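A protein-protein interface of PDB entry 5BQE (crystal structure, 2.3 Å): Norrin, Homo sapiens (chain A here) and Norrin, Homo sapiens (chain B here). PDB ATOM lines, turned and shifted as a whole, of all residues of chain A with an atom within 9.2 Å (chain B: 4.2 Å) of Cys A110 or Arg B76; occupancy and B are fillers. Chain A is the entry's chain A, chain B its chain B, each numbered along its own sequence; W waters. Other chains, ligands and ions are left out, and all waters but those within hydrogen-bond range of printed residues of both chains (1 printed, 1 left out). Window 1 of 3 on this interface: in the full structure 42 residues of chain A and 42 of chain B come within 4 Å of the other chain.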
ATOM      1  N   CYS A  48       5.873  -1.757  -9.009  1.00  0.00           N
ATOM      2  CA  CYS A  48       6.707  -1.540  -7.872  1.00  0.00           C
ATOM      3  C   CYS A  48       7.322  -2.857  -7.447  1.00  0.00           C
ATOM      4  O   CYS A  48       6.779  -3.900  -7.699  1.00  0.00           O
ATOM      5  CB  CYS A  48       5.899  -0.931  -6.767  1.00  0.00           C
ATOM      6  SG  CYS A  48       5.364   0.726  -7.146  1.00  0.00           S
ATOM      7  N   SER A  52       2.835  -6.804  -2.486  1.00  0.00           N
ATOM      8  CA  SER A  52       1.739  -6.380  -1.651  1.00  0.00           C
ATOM      9  C   SER A  52       1.283  -7.510  -0.757  1.00  0.00           C
ATOM     10  O   SER A  52       1.457  -8.647  -1.072  1.00  0.00           O
ATOM     11  CB  SER A  52       0.598  -5.776  -2.458  1.00  0.00           C
ATOM     12  OG  SER A  52       0.101  -6.632  -3.430  1.00  0.00           O
ATOM     13  N   ARG A  53       0.728  -7.165   0.384  1.00  0.00           N
ATOM     14  CA  ARG A  53       0.243  -8.150   1.317  1.00  0.00           C
ATOM     15  C   ARG A  53      -0.873  -7.677   2.210  1.00  0.00           C
ATOM     16  O   ARG A  53      -1.148  -6.524   2.311  1.00  0.00           O
ATOM     17  CB  ARG A  53       1.379  -8.660   2.164  1.00  0.00           C
ATOM     18  CG  ARG A  53       2.021  -7.591   2.974  1.00  0.00           C
ATOM     19  CD  ARG A  53       3.158  -8.145   3.782  1.00  0.00           C
ATOM     20  NE  ARG A  53       3.455  -7.235   4.862  1.00  0.00           N
ATOM     21  CZ  ARG A  53       4.303  -6.231   4.758  1.00  0.00           C
ATOM     22  NH1 ARG A  53       4.516  -5.446   5.787  1.00  0.00           N
ATOM     23  NH2 ARG A  53       4.940  -6.023   3.627  1.00  0.00           N
ATOM     24  N   SER A  54      -1.522  -8.617   2.855  1.00  0.00           N
ATOM     25  CA  SER A  54      -2.569  -8.307   3.817  1.00  0.00           C
ATOM     26  C   SER A  54      -2.625  -9.395   4.884  1.00  0.00           C
ATOM     27  O   SER A  54      -2.673 -10.581   4.565  1.00  0.00           O
ATOM     28  CB  SER A  54      -3.922  -8.175   3.121  1.00  0.00           C
ATOM     29  OG  SER A  54      -4.912  -7.692   4.011  1.00  0.00           O
ATOM     30  N   GLU A  55      -2.623  -8.973   6.147  1.00  0.00           N
ATOM     31  CA  GLU A  55      -2.569  -9.884   7.284  1.00  0.00           C
ATOM     32  C   GLU A  55      -3.785  -9.689   8.180  1.00  0.00           C
ATOM     33  O   GLU A  55      -4.267  -8.568   8.325  1.00  0.00           O
ATOM     34  CB  GLU A  55      -1.292  -9.650   8.094  1.00  0.00           C
ATOM     35  CG  GLU A  55      -0.029 -10.230   7.474  1.00  0.00           C
ATOM     36  CD  GLU A  55       1.238  -9.630   8.057  1.00  0.00           C
ATOM     37  OE1 GLU A  55       1.152  -8.942   9.095  1.00  0.00           O
ATOM     38  OE2 GLU A  55       2.320  -9.848   7.472  1.00  0.00           O
ATOM     39  N   GLN A  66     -10.855  -2.999  12.184  1.00  0.00           N
ATOM     40  CA  GLN A  66     -10.422  -3.160  10.834  1.00  0.00           C
ATOM     41  C   GLN A  66      -9.787  -4.518  10.855  1.00  0.00           C
ATOM     42  O   GLN A  66      -8.846  -4.753  11.578  1.00  0.00           O
ATOM     43  CB  GLN A  66      -9.411  -2.086  10.505  1.00  0.00           C
ATOM     44  CG  GLN A  66      -8.514  -2.405   9.339  1.00  0.00           C
ATOM     45  CD  GLN A  66      -9.286  -2.728   8.084  1.00  0.00           C
ATOM     46  OE1 GLN A  66      -8.894  -3.604   7.305  1.00  0.00           O
ATOM     47  NE2 GLN A  66     -10.389  -2.013   7.872  1.00  0.00           N
ATOM     48  N   PHE A  68      -7.960  -6.287   8.761  1.00  0.00           N
ATOM     49  CA  PHE A  68      -6.685  -6.592   8.166  1.00  0.00           C
ATOM     50  C   PHE A  68      -5.722  -5.451   8.242  1.00  0.00           C
ATOM     51  O   PHE A  68      -6.107  -4.334   8.341  1.00  0.00           O
ATOM     52  CB  PHE A  68      -6.869  -6.970   6.715  1.00  0.00           C
ATOM     53  CG  PHE A  68      -7.828  -8.083   6.498  1.00  0.00           C
ATOM     54  CD1 PHE A  68      -7.451  -9.372   6.710  1.00  0.00           C
ATOM     55  CD2 PHE A  68      -9.091  -7.832   6.074  1.00  0.00           C
ATOM     56  CE1 PHE A  68      -8.320 -10.389   6.508  1.00  0.00           C
ATOM     57  CE2 PHE A  68      -9.974  -8.841   5.869  1.00  0.00           C
ATOM     58  CZ  PHE A  68      -9.587 -10.128   6.084  1.00  0.00           C
ATOM     59  N   ARG A  69      -4.453  -5.776   8.172  1.00  0.00           N
ATOM     60  CA  ARG A  69      -3.399  -4.812   8.117  1.00  0.00           C
ATOM     61  C   ARG A  69      -2.631  -5.080   6.851  1.00  0.00           C
ATOM     62  O   ARG A  69      -2.193  -6.166   6.637  1.00  0.00           O
ATOM     63  CB  ARG A  69      -2.487  -5.000   9.303  1.00  0.00           C
ATOM     64  CG  ARG A  69      -1.239  -4.160   9.255  1.00  0.00           C
ATOM     65  CD  ARG A  69      -0.058  -4.865   9.877  1.00  0.00           C
ATOM     66  NE  ARG A  69      -0.299  -5.240  11.261  1.00  0.00           N
ATOM     67  CZ  ARG A  69       0.230  -6.310  11.840  1.00  0.00           C
ATOM     68  NH1 ARG A  69       1.032  -7.105  11.148  1.00  0.00           N
ATOM     69  NH2 ARG A  69      -0.041  -6.586  13.105  1.00  0.00           N
ATOM     70  N   SER A  70      -2.474  -4.094   5.999  1.00  0.00           N
ATOM     71  CA  SER A  70      -1.914  -4.343   4.689  1.00  0.00           C
ATOM     72  C   SER A  70      -0.925  -3.337   4.141  1.00  0.00           C
ATOM     73  O   SER A  70      -0.890  -2.225   4.568  1.00  0.00           O
ATOM     74  CB  SER A  70      -3.039  -4.531   3.706  1.00  0.00           C
ATOM     75  OG  SER A  70      -3.881  -3.433   3.698  1.00  0.00           O
ATOM     76  N   SER A  71      -0.112  -3.759   3.191  1.00  0.00           N
ATOM     77  CA  SER A  71       0.816  -2.868   2.514  1.00  0.00           C
ATOM     78  C   SER A  71       0.754  -3.124   1.013  1.00  0.00           C
ATOM     79  O   SER A  71       0.716  -4.273   0.572  1.00  0.00           O
ATOM     80  CB  SER A  71       2.240  -3.068   3.034  1.00  0.00           C
ATOM     81  OG  SER A  71       3.196  -2.753   2.036  1.00  0.00           O
ATOM     82  N   CYS A  72       0.777  -2.059   0.230  1.00  0.00           N
ATOM     83  CA  CYS A  72       0.726  -2.155  -1.209  1.00  0.00           C
ATOM     84  C   CYS A  72       1.326  -0.945  -1.863  1.00  0.00           C
ATOM     85  O   CYS A  72       0.954   0.154  -1.563  1.00  0.00           O
ATOM     86  CB  CYS A  72      -0.711  -2.307  -1.652  1.00  0.00           C
ATOM     87  SG  CYS A  72      -0.991  -2.308  -3.406  1.00  0.00           S
ATOM     88  N   HIS A  73       2.248  -1.152  -2.777  1.00  0.00           N
ATOM     89  CA  HIS A  73       2.920  -0.044  -3.415  1.00  0.00           C
ATOM     90  C   HIS A  73       2.402   0.297  -4.804  1.00  0.00           C
ATOM     91  O   HIS A  73       2.228  -0.544  -5.625  1.00  0.00           O
ATOM     92  CB  HIS A  73       4.412  -0.291  -3.445  1.00  0.00           C
ATOM     93  CG  HIS A  73       5.102   0.059  -2.174  1.00  0.00           C
ATOM     94  ND1 HIS A  73       4.897  -0.624  -1.004  1.00  0.00           N
ATOM     95  CD2 HIS A  73       5.991   1.027  -1.888  1.00  0.00           C
ATOM     96  CE1 HIS A  73       5.624  -0.091  -0.050  1.00  0.00           C
ATOM     97  NE2 HIS A  73       6.302   0.910  -0.563  1.00  0.00           N
ATOM     98  N   CYS A  74       2.152   1.566  -5.043  1.00  0.00           N
ATOM     99  CA  CYS A  74       1.576   2.010  -6.305  1.00  0.00           C
ATOM    100  C   CYS A  74       2.490   3.007  -7.000  1.00  0.00           C
ATOM    101  O   CYS A  74       3.072   3.882  -6.358  1.00  0.00           O
ATOM    102  CB  CYS A  74       0.207   2.647  -6.064  1.00  0.00           C
ATOM    103  SG  CYS A  74      -0.975   1.565  -5.227  1.00  0.00           S
ATOM    104  N   CYS A  75       2.606   2.877  -8.317  1.00  0.00           N
ATOM    105  CA  CYS A  75       3.399   3.808  -9.106  1.00  0.00           C
ATOM    106  C   CYS A  75       2.625   5.112  -9.236  1.00  0.00           C
ATOM    107  O   CYS A  75       1.539   5.143  -9.817  1.00  0.00           O
ATOM    108  CB  CYS A  75       3.718   3.219 -10.480  1.00  0.00           C
ATOM    109  SG  CYS A  75       4.898   4.187 -11.452  1.00  0.00           S
ATOM    110  N   ARG A  76       3.182   6.182  -8.677  1.00  0.00           N
ATOM    111  CA  ARG A  76       2.486   7.460  -8.592  1.00  0.00           C
ATOM    112  C   ARG A  76       3.424   8.639  -8.830  1.00  0.00           C
ATOM    113  O   ARG A  76       4.634   8.512  -8.655  1.00  0.00           O
ATOM    114  CB  ARG A  76       1.825   7.597  -7.223  1.00  0.00           C
ATOM    115  CG  ARG A  76       0.613   6.713  -7.041  1.00  0.00           C
ATOM    116  CD  ARG A  76      -0.017   6.939  -5.684  1.00  0.00           C
ATOM    117  NE  ARG A  76      -1.176   6.081  -5.456  1.00  0.00           N
ATOM    118  CZ  ARG A  76      -1.679   5.812  -4.256  1.00  0.00           C
ATOM    119  NH1 ARG A  76      -1.122   6.325  -3.165  1.00  0.00           N
ATOM    120  NH2 ARG A  76      -2.736   5.020  -4.140  1.00  0.00           N
ATOM    121  N   CYS A 107       7.226   4.887  -6.017  1.00  0.00           N
ATOM    122  CA  CYS A 107       6.358   3.879  -5.428  1.00  0.00           C
ATOM    123  C   CYS A 107       6.019   4.232  -3.990  1.00  0.00           C
ATOM    124  O   CYS A 107       6.907   4.303  -3.141  1.00  0.00           O
ATOM    125  CB  CYS A 107       7.030   2.508  -5.488  1.00  0.00           C
ATOM    126  SG  CYS A 107       7.084   1.781  -7.140  1.00  0.00           S
ATOM    127  N   GLU A 108       4.737   4.466  -3.723  1.00  0.00           N
ATOM    128  CA  GLU A 108       4.283   4.782  -2.373  1.00  0.00           C
ATOM    129  C   GLU A 108       3.092   3.920  -1.968  1.00  0.00           C
ATOM    130  O   GLU A 108       2.360   3.403  -2.816  1.00  0.00           O
ATOM    131  CB  GLU A 108       3.919   6.269  -2.256  1.00  0.00           C
ATOM    132  CG  GLU A 108       2.793   6.733  -3.182  1.00  0.00           C
ATOM    133  CD  GLU A 108       2.269   8.118  -2.833  1.00  0.00           C
ATOM    134  OE1 GLU A 108       3.028   8.925  -2.259  1.00  0.00           O
ATOM    135  OE2 GLU A 108       1.089   8.395  -3.129  1.00  0.00           O
ATOM    136  N   GLU A 109       2.918   3.774  -0.657  1.00  0.00           N
ATOM    137  CA  GLU A 109       1.824   2.998  -0.091  1.00  0.00           C
ATOM    138  C   GLU A 109       0.482   3.436  -0.653  1.00  0.00           C
ATOM    139  O   GLU A 109       0.240   4.627  -0.852  1.00  0.00           O
ATOM    140  CB  GLU A 109       1.822   3.125   1.434  1.00  0.00           C
ATOM    141  CG  GLU A 109       2.799   2.199   2.141  1.00  0.00           C
ATOM    142  CD  GLU A 109       2.445   0.728   1.982  1.00  0.00           C
ATOM    143  OE1 GLU A 109       1.304   0.424   1.572  1.00  0.00           O
ATOM    144  OE2 GLU A 109       3.312  -0.124   2.271  1.00  0.00           O
ATOM    145  N   CYS A 110      -0.376   2.456  -0.913  1.00  0.00           N
ATOM    146  CA  CYS A 110      -1.711   2.709  -1.433  1.00  0.00           C
ATOM    147  C   CYS A 110      -2.479   3.675  -0.540  1.00  0.00           C
ATOM    148  O   CYS A 110      -2.951   4.712  -1.003  1.00  0.00           O
ATOM    149  CB  CYS A 110      -2.476   1.389  -1.568  1.00  0.00           C
ATOM    150  SG  CYS A 110      -4.267   1.578  -1.674  1.00  0.00           S
ATOM    151  N   ASN A 111      -2.589   3.333   0.738  1.00  0.00           N
ATOM    152  CA  ASN A 111      -3.367   4.123   1.680  1.00  0.00           C
ATOM    153  C   ASN A 111      -2.461   4.903   2.636  1.00  0.00           C
ATOM    154  O   ASN A 111      -2.655   4.900   3.851  1.00  0.00           O
ATOM    155  CB  ASN A 111      -4.332   3.205   2.441  1.00  0.00           C
ATOM    156  CG  ASN A 111      -5.787   3.554   2.189  1.00  0.00           C
ATOM    157  OD1 ASN A 111      -6.470   4.093   3.061  1.00  0.00           O
ATOM    158  ND2 ASN A 111      -6.269   3.248   0.989  1.00  0.00           N
ATOM    159  N   SER A 112      -1.458   5.576   2.075  1.00  0.00           N
ATOM    160  CA  SER A 112      -0.562   6.416   2.866  1.00  0.00           C
ATOM    161  C   SER A 112       0.279   7.319   1.965  1.00  0.00           C
ATOM    162  O   SER A 112      -0.210   7.847   0.965  1.00  0.00           O
ATOM    163  CB  SER A 112       0.352   5.559   3.746  1.00  0.00           C
ATOM    164  OG  SER A 112      -0.394   4.738   4.628  1.00  0.00           O
ATOM    165  N   CYS B  44      -2.456 -12.822   2.589  1.00  0.00           N
ATOM    166  CA  CYS B  44      -2.291 -12.644   1.157  1.00  0.00           C
ATOM    167  C   CYS B  44      -0.954 -11.955   0.919  1.00  0.00           C
ATOM    168  O   CYS B  44      -0.595 -11.040   1.650  1.00  0.00           O
ATOM    169  CB  CYS B  44      -3.437 -11.818   0.571  1.00  0.00           C
ATOM    170  SG  CYS B  44      -5.063 -12.554   0.783  1.00  0.00           S
ATOM    171  N   CYS B  74      -3.725  -4.361  -5.611  1.00  0.00           N
ATOM    172  CA  CYS B  74      -3.123  -4.859  -4.400  1.00  0.00           C
ATOM    173  C   CYS B  74      -3.590  -6.264  -4.094  1.00  0.00           C
ATOM    174  O   CYS B  74      -4.702  -6.576  -4.363  1.00  0.00           O
ATOM    175  CB  CYS B  74      -3.496  -3.942  -3.262  1.00  0.00           C
ATOM    176  SG  CYS B  74      -2.981  -2.252  -3.512  1.00  0.00           S
ATOM    177  N   CYS B  75      -2.726  -7.093  -3.533  1.00  0.00           N
ATOM    178  CA  CYS B  75      -3.071  -8.446  -3.133  1.00  0.00           C
ATOM    179  C   CYS B  75      -3.804  -8.437  -1.810  1.00  0.00           C
ATOM    180  O   CYS B  75      -3.254  -8.103  -0.807  1.00  0.00           O
ATOM    181  CB  CYS B  75      -1.824  -9.321  -3.054  1.00  0.00           C
ATOM    182  SG  CYS B  75      -2.048 -11.087  -2.833  1.00  0.00           S
ATOM    183  N   ARG B  76      -5.063  -8.803  -1.842  1.00  0.00           N
ATOM    184  CA  ARG B  76      -5.930  -8.690  -0.673  1.00  0.00           C
ATOM    185  C   ARG B  76      -6.813  -9.924  -0.485  1.00  0.00           C
ATOM    186  O   ARG B  76      -6.986 -10.715  -1.411  1.00  0.00           O
ATOM    187  CB  ARG B  76      -6.815  -7.451  -0.798  1.00  0.00           C
ATOM    188  CG  ARG B  76      -6.083  -6.129  -0.688  1.00  0.00           C
ATOM    189  CD  ARG B  76      -7.043  -4.999  -0.978  1.00  0.00           C
ATOM    190  NE  ARG B  76      -6.445  -3.681  -0.807  1.00  0.00           N
ATOM    191  CZ  ARG B  76      -6.999  -2.558  -1.251  1.00  0.00           C
ATOM    192  NH1 ARG B  76      -8.161  -2.602  -1.890  1.00  0.00           N
ATOM    193  NH2 ARG B  76      -6.397  -1.392  -1.060  1.00  0.00           N
ATOM    194  N   PRO B  77      -7.381 -10.085   0.720  1.00  0.00           N
ATOM    195  CA  PRO B  77      -8.371 -11.141   0.954  1.00  0.00           C
ATOM    196  C   PRO B  77      -9.597 -10.960   0.074  1.00  0.00           C
ATOM    197  O   PRO B  77     -10.156  -9.864   0.032  1.00  0.00           O
ATOM    198  CB  PRO B  77      -8.742 -10.963   2.429  1.00  0.00           C
ATOM    199  CG  PRO B  77      -7.626 -10.176   3.026  1.00  0.00           C
ATOM    200  CD  PRO B  77      -7.128  -9.292   1.934  1.00  0.00           C
ATOM    201  N   GLN B  78     -10.009 -12.018  -0.616  1.00  0.00           N
ATOM    202  CA  GLN B  78     -11.213 -11.973  -1.432  1.00  0.00           C
ATOM    203  C   GLN B  78     -12.372 -12.557  -0.632  1.00  0.00           C
ATOM    204  O   GLN B  78     -13.462 -11.983  -0.576  1.00  0.00           O
ATOM    205  CB  GLN B  78     -11.015 -12.739  -2.740  1.00  0.00           C
ATOM    206  CG  GLN B  78     -12.215 -12.644  -3.657  1.00  0.00           C
ATOM    207  CD  GLN B  78     -12.011 -13.317  -4.997  1.00  0.00           C
ATOM    208  OE1 GLN B  78     -11.372 -14.367  -5.092  1.00  0.00           O
ATOM    209  NE2 GLN B  78     -12.563 -12.714  -6.044  1.00  0.00           N
ATOM    210  N   CYS B 105      -7.388 -15.141  -1.980  1.00  0.00           N
ATOM    211  CA  CYS B 105      -6.812 -13.835  -2.253  1.00  0.00           C
ATOM    212  C   CYS B 105      -7.128 -13.442  -3.687  1.00  0.00           C
ATOM    213  O   CYS B 105      -7.354 -14.299  -4.540  1.00  0.00           O
ATOM    214  CB  CYS B 105      -5.296 -13.845  -2.024  1.00  0.00           C
ATOM    215  SG  CYS B 105      -4.798 -14.233  -0.336  1.00  0.00           S
ATOM    216  N   HIS B 106      -7.162 -12.141  -3.943  1.00  0.00           N
ATOM    217  CA  HIS B 106      -7.259 -11.648  -5.306  1.00  0.00           C
ATOM    218  C   HIS B 106      -6.598 -10.282  -5.412  1.00  0.00           C
ATOM    219  O   HIS B 106      -6.288  -9.649  -4.400  1.00  0.00           O
ATOM    220  CB  HIS B 106      -8.719 -11.577  -5.761  1.00  0.00           C
ATOM    221  CG  HIS B 106      -9.495 -10.459  -5.141  1.00  0.00           C
ATOM    222  ND1 HIS B 106      -9.204  -9.942  -3.898  1.00  0.00           N
ATOM    223  CD2 HIS B 106     -10.556  -9.754  -5.600  1.00  0.00           C
ATOM    224  CE1 HIS B 106     -10.050  -8.972  -3.613  1.00  0.00           C
ATOM    225  NE2 HIS B 106     -10.885  -8.836  -4.635  1.00  0.00           N
ATOM    226  N   GLU B 108      -6.899  -6.497  -6.209  1.00  0.00           N
ATOM    227  CA  GLU B 108      -8.003  -5.555  -6.093  1.00  0.00           C
ATOM    228  C   GLU B 108      -7.524  -4.123  -6.264  1.00  0.00           C
ATOM    229  O   GLU B 108      -6.410  -3.783  -5.867  1.00  0.00           O
ATOM    230  CB  GLU B 108      -8.682  -5.720  -4.735  1.00  0.00           C
ATOM    231  CG  GLU B 108      -9.932  -4.881  -4.542  1.00  0.00           C
ATOM    232  CD  GLU B 108     -10.548  -5.071  -3.169  1.00  0.00           C
ATOM    233  OE1 GLU B 108      -9.810  -5.429  -2.228  1.00  0.00           O
ATOM    234  OE2 GLU B 108     -11.774  -4.871  -3.031  1.00  0.00           O
ATOM    235  N   GLU B 109      -8.378  -3.287  -6.845  1.00  0.00           N
ATOM    236  CA  GLU B 109      -8.067  -1.876  -7.038  1.00  0.00           C
ATOM    237  C   GLU B 109      -7.779  -1.216  -5.698  1.00  0.00           C
ATOM    238  O   GLU B 109      -8.536  -1.381  -4.743  1.00  0.00           O
ATOM    239  CB  GLU B 109      -9.225  -1.169  -7.741  1.00  0.00           C
ATOM    240  CG  GLU B 109      -8.865   0.175  -8.326  1.00  0.00           C
ATOM    241  CD  GLU B 109      -7.793   0.070  -9.389  1.00  0.00           C
ATOM    242  OE1 GLU B 109      -6.696   0.623  -9.179  1.00  0.00           O
ATOM    243  OE2 GLU B 109      -8.049  -0.568 -10.430  1.00  0.00           O
ATOM    244  N   CYS B 110      -6.683  -0.467  -5.644  1.00  0.00           N
ATOM    245  CA  CYS B 110      -6.193   0.116  -4.400  1.00  0.00           C
ATOM    246  C   CYS B 110      -7.273   0.894  -3.647  1.00  0.00           C
ATOM    247  O   CYS B 110      -7.569   0.592  -2.489  1.00  0.00           O
ATOM    248  CB  CYS B 110      -4.999   1.025  -4.694  1.00  0.00           C
ATOM    249  SG  CYS B 110      -4.752   2.345  -3.491  1.00  0.00           S
ATOM    250  N   SER B 112     -10.992   1.450  -3.837  1.00  0.00           N
ATOM    251  CA  SER B 112     -12.237   0.961  -4.414  1.00  0.00           C
ATOM    252  C   SER B 112     -13.367   1.982  -4.300  1.00  0.00           C
ATOM    253  O   SER B 112     -13.129   3.180  -4.138  1.00  0.00           O
ATOM    254  CB  SER B 112     -12.641  -0.343  -3.722  1.00  0.00           C
ATOM    255  OG  SER B 112     -11.537  -0.925  -3.052  1.00  0.00           O
HETATM  256  O   HOH W   1      -4.043  -3.124   0.291  1.00  0.00           O
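Cys B74 touches Ser A52 (C to OG, 3.8 Å).
Arg A53 touches Cys B44.
Cys B75 touches Arg A53.
CB of Ser A54 touches O of Cys B75 (3.99 Å).
OG of Ser A54 touches CD of Pro B77, 3.4 Å away.
Phe A68 touches Pro B77 (CE1 to CG, 3.6 Å).
Water W1 bridges NE of Arg B76 (2.7 Å) and OG of Ser A70 (3.4 Å).
The side-chain amide nitrogen of Asn A111 is in hydrogen-bond range of the side-chain sulfur of Cys A110, 3.7 Å away.
O of Arg B76 lies within hydrogen-bond range of N of His B106 (2.9 Å).
NH1 of Arg B76 lies within salt-bridge range of OE1 of Glu B108, 3.3 Å away.
The side-chain carboxylate of Glu A108 lies within salt-bridge range of the guanidinium group of Arg A76 (3.0 Å).
The backbone carbonyl oxygen of Glu A109 sits at hydrogen-bond distance from the guanidinium group of Arg A76, 3.2 Å away.
The guanidinium group (NH2) of Arg B76 sits at hydrogen-bond distance from the backbone carbonyl oxygen (O) of Cys B110, at 2.7 Å.
SG of Cys B74 is disulfide-bonded to SG of Cys A72 (2.0 Å).
The guanidinium group (NH2) of Arg A76 lies within hydrogen-bond range of the side-chain sulfur (SG) of Cys B110 (3.4 Å).
The side-chain sulfur (SG) of Cys A110 forms a disulfide with the side-chain sulfur (SG) of Cys B110.
NH2 of Arg B76 sits at hydrogen-bond distance from SG of Cys A110, at 3.7 Å.
The backbone NH of Ser A54 lies within hydrogen-bond range of the backbone carbonyl oxygen of Cys B44, at 2.9 Å.
N of Cys B75 sits at hydrogen-bond distance from OG of Ser A52 (2.9 Å).
Hydrophobic or aromatic side chains of chain A within 4 Å of the printed part of chain B: Phe A68.
Hydrophobic or aromatic side chains of chain B that line the printed part of chain A: Pro B77.
Along chain B the printed residues that touch a printed residue of chain A span positions 44 to 110.
Among the printed residues, 12 pairs touch across the chains.
Among the printed residues, no Asp or Glu carboxylate lies within 4 Å of a Lys or Arg side-chain nitrogen of the other chain.
Of the printed residues of chain B, Cys A110 touches Arg B76 (3.7 Å) and Cys B110 (2.0 Å).
Arg B76 touches one residue of chain A.
Pro B77 touches just these residues of chain A: Ser A54 and Phe A68.
Cys B110 touches two residues of chain A.
Of the printed residues of chain B, Cys A72 touches Cys B74.
Of the printed residues of chain A, Cys B74 touches Ser A52 and Cys A72.
Glu A109 touches none of the printed residues of chain B.
Ser A70 touches none of the printed residues of chain B.
The nearest printed residue of chain B that does not touch Cys A110 is Cys B74 (4.2 Å).
The nearest residue of chain A that does not touch Arg B76 is Ser A54 (4.3 Å).
The nearest printed residue of chain A that does not touch Cys B74 is Cys A110 (4.2 Å).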
